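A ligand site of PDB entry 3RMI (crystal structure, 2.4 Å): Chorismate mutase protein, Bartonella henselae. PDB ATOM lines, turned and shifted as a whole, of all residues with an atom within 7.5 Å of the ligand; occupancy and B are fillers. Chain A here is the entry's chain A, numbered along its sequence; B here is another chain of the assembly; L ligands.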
ATOM      1  N   ARG A  35      -1.312  27.536   8.144  1.00  0.00           N
ATOM      2  CA  ARG A  35      -1.819  27.639   6.762  1.00  0.00           C
ATOM      3  C   ARG A  35      -0.946  26.822   5.830  1.00  0.00           C
ATOM      4  O   ARG A  35      -1.458  26.134   4.934  1.00  0.00           O
ATOM      5  CB  ARG A  35      -1.785  29.072   6.279  1.00  0.00           C
ATOM      6  CG  ARG A  35      -2.667  29.323   5.031  1.00  0.00           C
ATOM      7  CD  ARG A  35      -2.331  30.657   4.442  1.00  0.00           C
ATOM      8  NE  ARG A  35      -3.237  31.104   3.397  1.00  0.00           N
ATOM      9  CZ  ARG A  35      -3.217  30.667   2.133  1.00  0.00           C
ATOM     10  NH1 ARG A  35      -2.389  29.699   1.745  1.00  0.00           N
ATOM     11  NH2 ARG A  35      -4.052  31.167   1.261  1.00  0.00           N
ATOM     12  N   CYS A  38      -1.486  23.188   6.030  1.00  0.00           N
ATOM     13  CA  CYS A  38      -2.635  22.796   5.192  1.00  0.00           C
ATOM     14  C   CYS A  38      -2.305  22.765   3.736  1.00  0.00           C
ATOM     15  O   CYS A  38      -2.594  21.792   3.074  1.00  0.00           O
ATOM     16  CB  CYS A  38      -3.820  23.735   5.360  1.00  0.00           C
ATOM     17  SG  CYS A  38      -4.641  23.472   6.867  1.00  0.00           S
ATOM     18  N   THR A  39      -1.701  23.834   3.224  1.00  0.00           N
ATOM     19  CA  THR A  39      -1.397  23.869   1.797  1.00  0.00           C
ATOM     20  C   THR A  39      -0.378  22.822   1.420  1.00  0.00           C
ATOM     21  O   THR A  39      -0.316  22.432   0.259  1.00  0.00           O
ATOM     22  CB  THR A  39      -0.903  25.224   1.303  1.00  0.00           C
ATOM     23  OG1 THR A  39       0.264  25.614   2.054  1.00  0.00           O
ATOM     24  CG2 THR A  39      -1.996  26.262   1.413  1.00  0.00           C
ATOM     25  N   ILE A  42      -2.390  19.795   0.921  1.00  0.00           N
ATOM     26  CA  ILE A  42      -2.975  19.923  -0.426  1.00  0.00           C
ATOM     27  C   ILE A  42      -1.941  19.586  -1.489  1.00  0.00           C
ATOM     28  O   ILE A  42      -2.252  18.884  -2.444  1.00  0.00           O
ATOM     29  CB  ILE A  42      -3.602  21.330  -0.710  1.00  0.00           C
ATOM     30  CG1 ILE A  42      -4.830  21.534   0.190  1.00  0.00           C
ATOM     31  CG2 ILE A  42      -4.002  21.479  -2.216  1.00  0.00           C
ATOM     32  CD1 ILE A  42      -5.443  22.945   0.111  1.00  0.00           C
ATOM     33  N   GLY A  43      -0.703  20.059  -1.337  1.00  0.00           N
ATOM     34  CA  GLY A  43       0.349  19.767  -2.319  1.00  0.00           C
ATOM     35  C   GLY A  43       0.610  18.264  -2.525  1.00  0.00           C
ATOM     36  O   GLY A  43       0.797  17.797  -3.670  1.00  0.00           O
ATOM     37  N   LYS A  46      -2.443  16.814  -4.311  1.00  0.00           N
ATOM     38  CA  LYS A  46      -2.410  17.179  -5.725  1.00  0.00           C
ATOM     39  C   LYS A  46      -1.370  16.357  -6.453  1.00  0.00           C
ATOM     40  O   LYS A  46      -1.636  15.851  -7.524  1.00  0.00           O
ATOM     41  CB  LYS A  46      -2.134  18.666  -5.943  1.00  0.00           C
ATOM     42  CG  LYS A  46      -3.285  19.631  -5.550  1.00  0.00           C
ATOM     43  CD  LYS A  46      -2.917  21.059  -5.923  1.00  0.00           C
ATOM     44  CE  LYS A  46      -4.044  22.021  -5.709  1.00  0.00           C
ATOM     45  NZ  LYS A  46      -3.734  23.345  -6.385  1.00  0.00           N
ATOM     46  N   PRO A  52      -3.133  19.991 -10.867  1.00  0.00           N
ATOM     47  CA  PRO A  52      -2.164  21.019 -11.204  1.00  0.00           C
ATOM     48  C   PRO A  52      -1.964  21.994 -10.036  1.00  0.00           C
ATOM     49  O   PRO A  52      -2.884  22.169  -9.234  1.00  0.00           O
ATOM     50  CB  PRO A  52      -2.837  21.721 -12.388  1.00  0.00           C
ATOM     51  CG  PRO A  52      -4.329  21.728 -11.945  1.00  0.00           C
ATOM     52  CD  PRO A  52      -4.512  20.442 -11.124  1.00  0.00           C
ATOM     53  N   ALA A  53      -0.775  22.581  -9.960  1.00  0.00           N
ATOM     54  CA  ALA A  53      -0.431  23.566  -8.942  1.00  0.00           C
ATOM     55  C   ALA A  53      -1.357  24.773  -8.986  1.00  0.00           C
ATOM     56  O   ALA A  53      -1.921  25.168  -7.964  1.00  0.00           O
ATOM     57  CB  ALA A  53       1.015  24.031  -9.113  1.00  0.00           C
ATOM     58  N   VAL A  54      -1.512  25.358 -10.171  1.00  0.00           N
ATOM     59  CA  VAL A  54      -2.415  26.506 -10.328  1.00  0.00           C
ATOM     60  C   VAL A  54      -3.818  26.013 -10.669  1.00  0.00           C
ATOM     61  O   VAL A  54      -4.058  25.351 -11.691  1.00  0.00           O
ATOM     62  CB  VAL A  54      -1.931  27.500 -11.403  1.00  0.00           C
ATOM     63  CG1 VAL A  54      -2.843  28.731 -11.397  1.00  0.00           C
ATOM     64  CG2 VAL A  54      -0.459  27.871 -11.152  1.00  0.00           C
ATOM     65  N   ASP A  55      -4.744  26.356  -9.798  1.00  0.00           N
ATOM     66  CA  ASP A  55      -6.144  25.993  -9.903  1.00  0.00           C
ATOM     67  C   ASP A  55      -6.946  27.311 -10.047  1.00  0.00           C
ATOM     68  O   ASP A  55      -7.339  27.904  -9.045  1.00  0.00           O
ATOM     69  CB  ASP A  55      -6.498  25.251  -8.628  1.00  0.00           C
ATOM     70  CG  ASP A  55      -7.860  24.615  -8.651  1.00  0.00           C
ATOM     71  OD1 ASP A  55      -8.783  25.175  -9.281  1.00  0.00           O
ATOM     72  OD2 ASP A  55      -7.987  23.547  -7.982  1.00  0.00           O
ATOM     73  N   ARG A  58     -10.232  28.102  -8.160  1.00  0.00           N
ATOM     74  CA  ARG A  58      -9.948  28.233  -6.708  1.00  0.00           C
ATOM     75  C   ARG A  58      -9.364  29.623  -6.361  1.00  0.00           C
ATOM     76  O   ARG A  58      -9.843  30.304  -5.446  1.00  0.00           O
ATOM     77  CB  ARG A  58      -9.023  27.086  -6.253  1.00  0.00           C
ATOM     78  CG  ARG A  58      -8.448  27.193  -4.847  1.00  0.00           C
ATOM     79  CD  ARG A  58      -9.510  27.154  -3.760  1.00  0.00           C
ATOM     80  NE  ARG A  58      -8.863  27.257  -2.451  1.00  0.00           N
ATOM     81  CZ  ARG A  58      -9.432  27.673  -1.332  1.00  0.00           C
ATOM     82  NH1 ARG A  58     -10.715  28.025  -1.288  1.00  0.00           N
ATOM     83  NH2 ARG A  58      -8.718  27.707  -0.203  1.00  0.00           N
ATOM     84  N   GLU A  59      -8.345  30.029  -7.117  1.00  0.00           N
ATOM     85  CA  GLU A  59      -7.626  31.305  -6.925  1.00  0.00           C
ATOM     86  C   GLU A  59      -8.606  32.450  -6.996  1.00  0.00           C
ATOM     87  O   GLU A  59      -8.601  33.339  -6.161  1.00  0.00           O
ATOM     88  CB  GLU A  59      -6.555  31.496  -8.021  1.00  0.00           C
ATOM     89  CG  GLU A  59      -5.083  31.661  -7.601  1.00  0.00           C
ATOM     90  CD  GLU A  59      -4.150  30.416  -7.912  1.00  0.00           C
ATOM     91  OE1 GLU A  59      -4.340  29.278  -7.367  1.00  0.00           O
ATOM     92  OE2 GLU A  59      -3.172  30.635  -8.701  1.00  0.00           O
ATOM     93  N   GLN A  62     -10.888  32.656  -3.929  1.00  0.00           N
ATOM     94  CA  GLN A  62     -10.181  33.087  -2.720  1.00  0.00           C
ATOM     95  C   GLN A  62     -10.023  34.619  -2.770  1.00  0.00           C
ATOM     96  O   GLN A  62     -10.200  35.286  -1.779  1.00  0.00           O
ATOM     97  CB  GLN A  62      -8.817  32.419  -2.599  1.00  0.00           C
ATOM     98  CG  GLN A  62      -8.754  30.910  -2.407  1.00  0.00           C
ATOM     99  CD  GLN A  62      -7.321  30.427  -2.284  1.00  0.00           C
ATOM    100  OE1 GLN A  62      -6.749  30.484  -1.194  1.00  0.00           O
ATOM    101  NE2 GLN A  62      -6.724  29.956  -3.368  1.00  0.00           N
ATOM    102  N   LEU A  84      -2.763  38.165  -0.460  1.00  0.00           N
ATOM    103  CA  LEU A  84      -3.120  36.798  -0.792  1.00  0.00           C
ATOM    104  C   LEU A  84      -2.296  36.273  -1.980  1.00  0.00           C
ATOM    105  O   LEU A  84      -1.829  35.128  -1.968  1.00  0.00           O
ATOM    106  CB  LEU A  84      -4.609  36.716  -1.083  1.00  0.00           C
ATOM    107  CG  LEU A  84      -5.195  35.360  -1.465  1.00  0.00           C
ATOM    108  CD1 LEU A  84      -5.049  34.316  -0.362  1.00  0.00           C
ATOM    109  CD2 LEU A  84      -6.664  35.568  -1.832  1.00  0.00           C
ATOM    110  N   ILE A  87       1.041  35.210  -0.851  1.00  0.00           N
ATOM    111  CA  ILE A  87       1.006  33.895  -0.223  1.00  0.00           C
ATOM    112  C   ILE A  87       0.847  32.789  -1.292  1.00  0.00           C
ATOM    113  O   ILE A  87       1.536  31.768  -1.250  1.00  0.00           O
ATOM    114  CB  ILE A  87      -0.118  33.786   0.801  1.00  0.00           C
ATOM    115  CG1 ILE A  87       0.102  34.793   1.931  1.00  0.00           C
ATOM    116  CG2 ILE A  87      -0.146  32.411   1.389  1.00  0.00           C
ATOM    117  CD1 ILE A  87       1.413  34.563   2.702  1.00  0.00           C
ATOM    118  N   ILE A  88      -0.028  33.015  -2.255  1.00  0.00           N
ATOM    119  CA  ILE A  88      -0.339  31.961  -3.233  1.00  0.00           C
ATOM    120  C   ILE A  88       0.858  31.640  -4.094  1.00  0.00           C
ATOM    121  O   ILE A  88       1.039  30.500  -4.509  1.00  0.00           O
ATOM    122  CB  ILE A  88      -1.490  32.362  -4.128  1.00  0.00           C
ATOM    123  CG1 ILE A  88      -2.806  32.309  -3.359  1.00  0.00           C
ATOM    124  CG2 ILE A  88      -1.526  31.490  -5.411  1.00  0.00           C
ATOM    125  CD1 ILE A  88      -3.998  32.873  -4.227  1.00  0.00           C
ATOM    126  N   LYS A  89       1.673  32.640  -4.381  1.00  0.00           N
ATOM    127  CA  LYS A  89       2.906  32.421  -5.176  1.00  0.00           C
ATOM    128  C   LYS A  89       3.861  31.455  -4.448  1.00  0.00           C
ATOM    129  O   LYS A  89       4.491  30.590  -5.069  1.00  0.00           O
ATOM    130  CB  LYS A  89       3.585  33.782  -5.412  1.00  0.00           C
ATOM    131  CG  LYS A  89       4.600  33.848  -6.533  1.00  0.00           C
ATOM    132  CD  LYS A  89       5.385  35.176  -6.476  1.00  0.00           C
ATOM    133  CE  LYS A  89       6.559  35.184  -7.458  1.00  0.00           C
ATOM    134  NZ  LYS A  89       7.541  36.257  -7.063  1.00  0.00           N
ATOM    135  N   VAL A  91       2.832  29.245  -2.257  1.00  0.00           N
ATOM    136  CA  VAL A  91       2.110  27.961  -2.238  1.00  0.00           C
ATOM    137  C   VAL A  91       2.281  27.215  -3.555  1.00  0.00           C
ATOM    138  O   VAL A  91       2.515  26.004  -3.557  1.00  0.00           O
ATOM    139  CB  VAL A  91       0.616  28.162  -1.931  1.00  0.00           C
ATOM    140  CG1 VAL A  91      -0.162  26.864  -2.169  1.00  0.00           C
ATOM    141  CG2 VAL A  91       0.430  28.642  -0.482  1.00  0.00           C
ATOM    142  N   VAL A  92       2.200  27.937  -4.660  1.00  0.00           N
ATOM    143  CA  VAL A  92       2.304  27.334  -5.979  1.00  0.00           C
ATOM    144  C   VAL A  92       3.721  26.777  -6.161  1.00  0.00           C
ATOM    145  O   VAL A  92       3.892  25.652  -6.651  1.00  0.00           O
ATOM    146  CB  VAL A  92       1.905  28.350  -7.081  1.00  0.00           C
ATOM    147  CG1 VAL A  92       2.484  27.959  -8.397  1.00  0.00           C
ATOM    148  CG2 VAL A  92       0.371  28.495  -7.156  1.00  0.00           C
ATOM    149  N   HIS A  95       3.856  23.603  -4.122  1.00  0.00           N
ATOM    150  CA  HIS A  95       3.153  22.524  -4.797  1.00  0.00           C
ATOM    151  C   HIS A  95       4.010  21.911  -5.889  1.00  0.00           C
ATOM    152  O   HIS A  95       4.037  20.703  -6.045  1.00  0.00           O
ATOM    153  CB  HIS A  95       1.845  23.044  -5.396  1.00  0.00           C
ATOM    154  CG  HIS A  95       0.747  23.247  -4.394  1.00  0.00           C
ATOM    155  ND1 HIS A  95      -0.505  23.687  -4.736  1.00  0.00           N
ATOM    156  CD2 HIS A  95       0.716  23.027  -3.063  1.00  0.00           C
ATOM    157  CE1 HIS A  95      -1.260  23.747  -3.658  1.00  0.00           C
ATOM    158  NE2 HIS A  95      -0.542  23.348  -2.624  1.00  0.00           N
ATOM    159  N   LEU B  14      -9.797  17.654   0.165  1.00  0.00           N
ATOM    160  CA  LEU B  14      -9.353  18.909  -0.398  1.00  0.00           C
ATOM    161  C   LEU B  14     -10.246  20.029   0.114  1.00  0.00           C
ATOM    162  O   LEU B  14      -9.747  21.054   0.587  1.00  0.00           O
ATOM    163  CB  LEU B  14      -9.426  18.784  -1.907  1.00  0.00           C
ATOM    164  CG  LEU B  14      -8.671  19.762  -2.800  1.00  0.00           C
ATOM    165  CD1 LEU B  14      -7.185  19.751  -2.456  1.00  0.00           C
ATOM    166  CD2 LEU B  14      -8.958  19.346  -4.284  1.00  0.00           C
ATOM    167  N   LEU B  17      -9.580  20.874   3.801  1.00  0.00           N
ATOM    168  CA  LEU B  17      -8.339  21.633   3.985  1.00  0.00           C
ATOM    169  C   LEU B  17      -8.511  23.067   3.509  1.00  0.00           C
ATOM    170  O   LEU B  17      -7.992  24.024   4.081  1.00  0.00           O
ATOM    171  CB  LEU B  17      -7.176  20.971   3.227  1.00  0.00           C
ATOM    172  CG  LEU B  17      -6.692  19.640   3.842  1.00  0.00           C
ATOM    173  CD1 LEU B  17      -6.052  18.777   2.780  1.00  0.00           C
ATOM    174  CD2 LEU B  17      -5.717  19.788   5.084  1.00  0.00           C
ATOM    175  N   ARG B  18      -9.299  23.235   2.481  1.00  0.00           N
ATOM    176  CA  ARG B  18      -9.532  24.580   1.999  1.00  0.00           C
ATOM    177  C   ARG B  18     -10.421  25.380   2.921  1.00  0.00           C
ATOM    178  O   ARG B  18     -10.286  26.601   2.978  1.00  0.00           O
ATOM    179  CB  ARG B  18     -10.069  24.544   0.595  1.00  0.00           C
ATOM    180  CG  ARG B  18      -8.975  24.187  -0.390  1.00  0.00           C
ATOM    181  CD  ARG B  18      -9.523  23.846  -1.766  1.00  0.00           C
ATOM    182  NE  ARG B  18      -8.468  23.822  -2.759  1.00  0.00           N
ATOM    183  CZ  ARG B  18      -8.616  23.447  -4.017  1.00  0.00           C
ATOM    184  NH1 ARG B  18      -9.792  23.024  -4.451  1.00  0.00           N
ATOM    185  NH2 ARG B  18      -7.589  23.485  -4.844  1.00  0.00           N
ATOM    186  N   ILE B  21      -7.820  26.807   5.385  1.00  0.00           N
ATOM    187  CA  ILE B  21      -7.055  27.853   4.724  1.00  0.00           C
ATOM    188  C   ILE B  21      -7.866  29.113   4.690  1.00  0.00           C
ATOM    189  O   ILE B  21      -7.402  30.179   5.076  1.00  0.00           O
ATOM    190  CB  ILE B  21      -6.657  27.396   3.324  1.00  0.00           C
ATOM    191  CG1 ILE B  21      -5.577  26.313   3.442  1.00  0.00           C
ATOM    192  CG2 ILE B  21      -6.155  28.593   2.489  1.00  0.00           C
ATOM    193  CD1 ILE B  21      -5.566  25.388   2.246  1.00  0.00           C
ATOM    194  N   ASP B  22      -9.098  28.988   4.231  1.00  0.00           N
ATOM    195  CA  ASP B  22      -9.977  30.154   4.079  1.00  0.00           C
ATOM    196  C   ASP B  22     -10.220  30.870   5.405  1.00  0.00           C
ATOM    197  O   ASP B  22     -10.241  32.096   5.477  1.00  0.00           O
ATOM    198  CB  ASP B  22     -11.276  29.717   3.431  1.00  0.00           C
ATOM    199  CG  ASP B  22     -11.130  29.431   1.920  1.00  0.00           C
ATOM    200  OD1 ASP B  22     -10.031  29.705   1.349  1.00  0.00           O
ATOM    201  OD2 ASP B  22     -12.135  28.979   1.292  1.00  0.00           O
ATOM    202  N   ASP B  25      -6.981  32.737   6.372  1.00  0.00           N
ATOM    203  CA  ASP B  25      -6.879  33.973   5.621  1.00  0.00           C
ATOM    204  C   ASP B  25      -7.734  35.100   6.198  1.00  0.00           C
ATOM    205  O   ASP B  25      -7.291  36.245   6.205  1.00  0.00           O
ATOM    206  CB  ASP B  25      -7.203  33.733   4.153  1.00  0.00           C
ATOM    207  CG  ASP B  25      -6.079  32.956   3.400  1.00  0.00           C
ATOM    208  OD1 ASP B  25      -4.937  32.870   3.935  1.00  0.00           O
ATOM    209  OD2 ASP B  25      -6.319  32.401   2.282  1.00  0.00           O
HETATM  210  C1  LIG L   1      -4.415  25.694  -3.132  1.00  0.00           C
HETATM  211  O1  LIG L   1      -4.724  24.826  -4.002  1.00  0.00           O
HETATM  212  O2  LIG L   1      -3.366  26.266  -3.358  1.00  0.00           O
HETATM  213  C2  LIG L   1      -5.232  25.997  -1.884  1.00  0.00           C
HETATM  214  O3  LIG L   1      -6.532  25.677  -2.287  1.00  0.00           O
HETATM  215  C3  LIG L   1      -5.363  27.376  -1.248  1.00  0.00           C
HETATM  216  C4  LIG L   1      -4.347  28.485  -1.584  1.00  0.00           C
HETATM  217  O4  LIG L   1      -4.142  28.886  -2.795  1.00  0.00           O
HETATM  218  O5  LIG L   1      -3.714  29.082  -0.662  1.00  0.00           O
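The side-chain carboxylate (OD2) of Asp 55 lies within salt-bridge range of the guanidinium group (NH2) of Arg 18 of chain B (3.2 Å). OG1 of Thr 39 lies within hydrogen-bond range of O of Arg 35. NE of Arg 35 lies within salt-bridge range of OD1 of Asp 25 of chain B, at 2.5 Å. The side-chain carboxylate (OD1) of Asp 55 is in hydrogen-bond range of the backbone NH (N) of Arg 58 (3.5 Å). The guanidinium group (NH2) of Arg 58 lies within salt-bridge range of the side-chain carboxylate (OD1) of Asp 22 of chain B (2.9 Å). The backbone carbonyl oxygen of Ala 53 lies within hydrogen-bond range of the side-chain amino group of Lys 46, 3.0 Å away. The backbone carbonyl oxygen of Pro 52 sits at hydrogen-bond distance from the side-chain amino group of Lys 46, at 3.2 Å. The backbone carbonyl oxygen (O) of Thr 39 sits at hydrogen-bond distance from a ring nitrogen (NE2) of His 95, 3.0 Å away.
NH2 of Arg 18 of chain B is in salt-bridge range of O1 of the ligand. An oxygen (O5) of the ligand lies within salt-bridge range of the guanidinium group of Arg 35 (2.8 Å). NE of Arg 58 sits at hydrogen-bond distance from O3 of the ligand (2.8 Å). O4 of the ligand sits at hydrogen-bond distance from NE2 of Gln 62 (2.9 Å). An oxygen (O1) of the ligand is in salt-bridge range of the side-chain amino group of Lys 46.
Residues that only touch the ligand: Thr 39 (3.9 Å), Ile 42 (3.7 Å), Ile 88 (3.7 Å), Val 91 (3.5 Å) and His 95 (3.3 Å). Hydrophobic or aromatic side chains that line the ligand: Ile 42, Ile 88, Val 91 and His 95. The nearest printed residue that does not touch the ligand is Ile 21 of chain B (4.01 Å).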
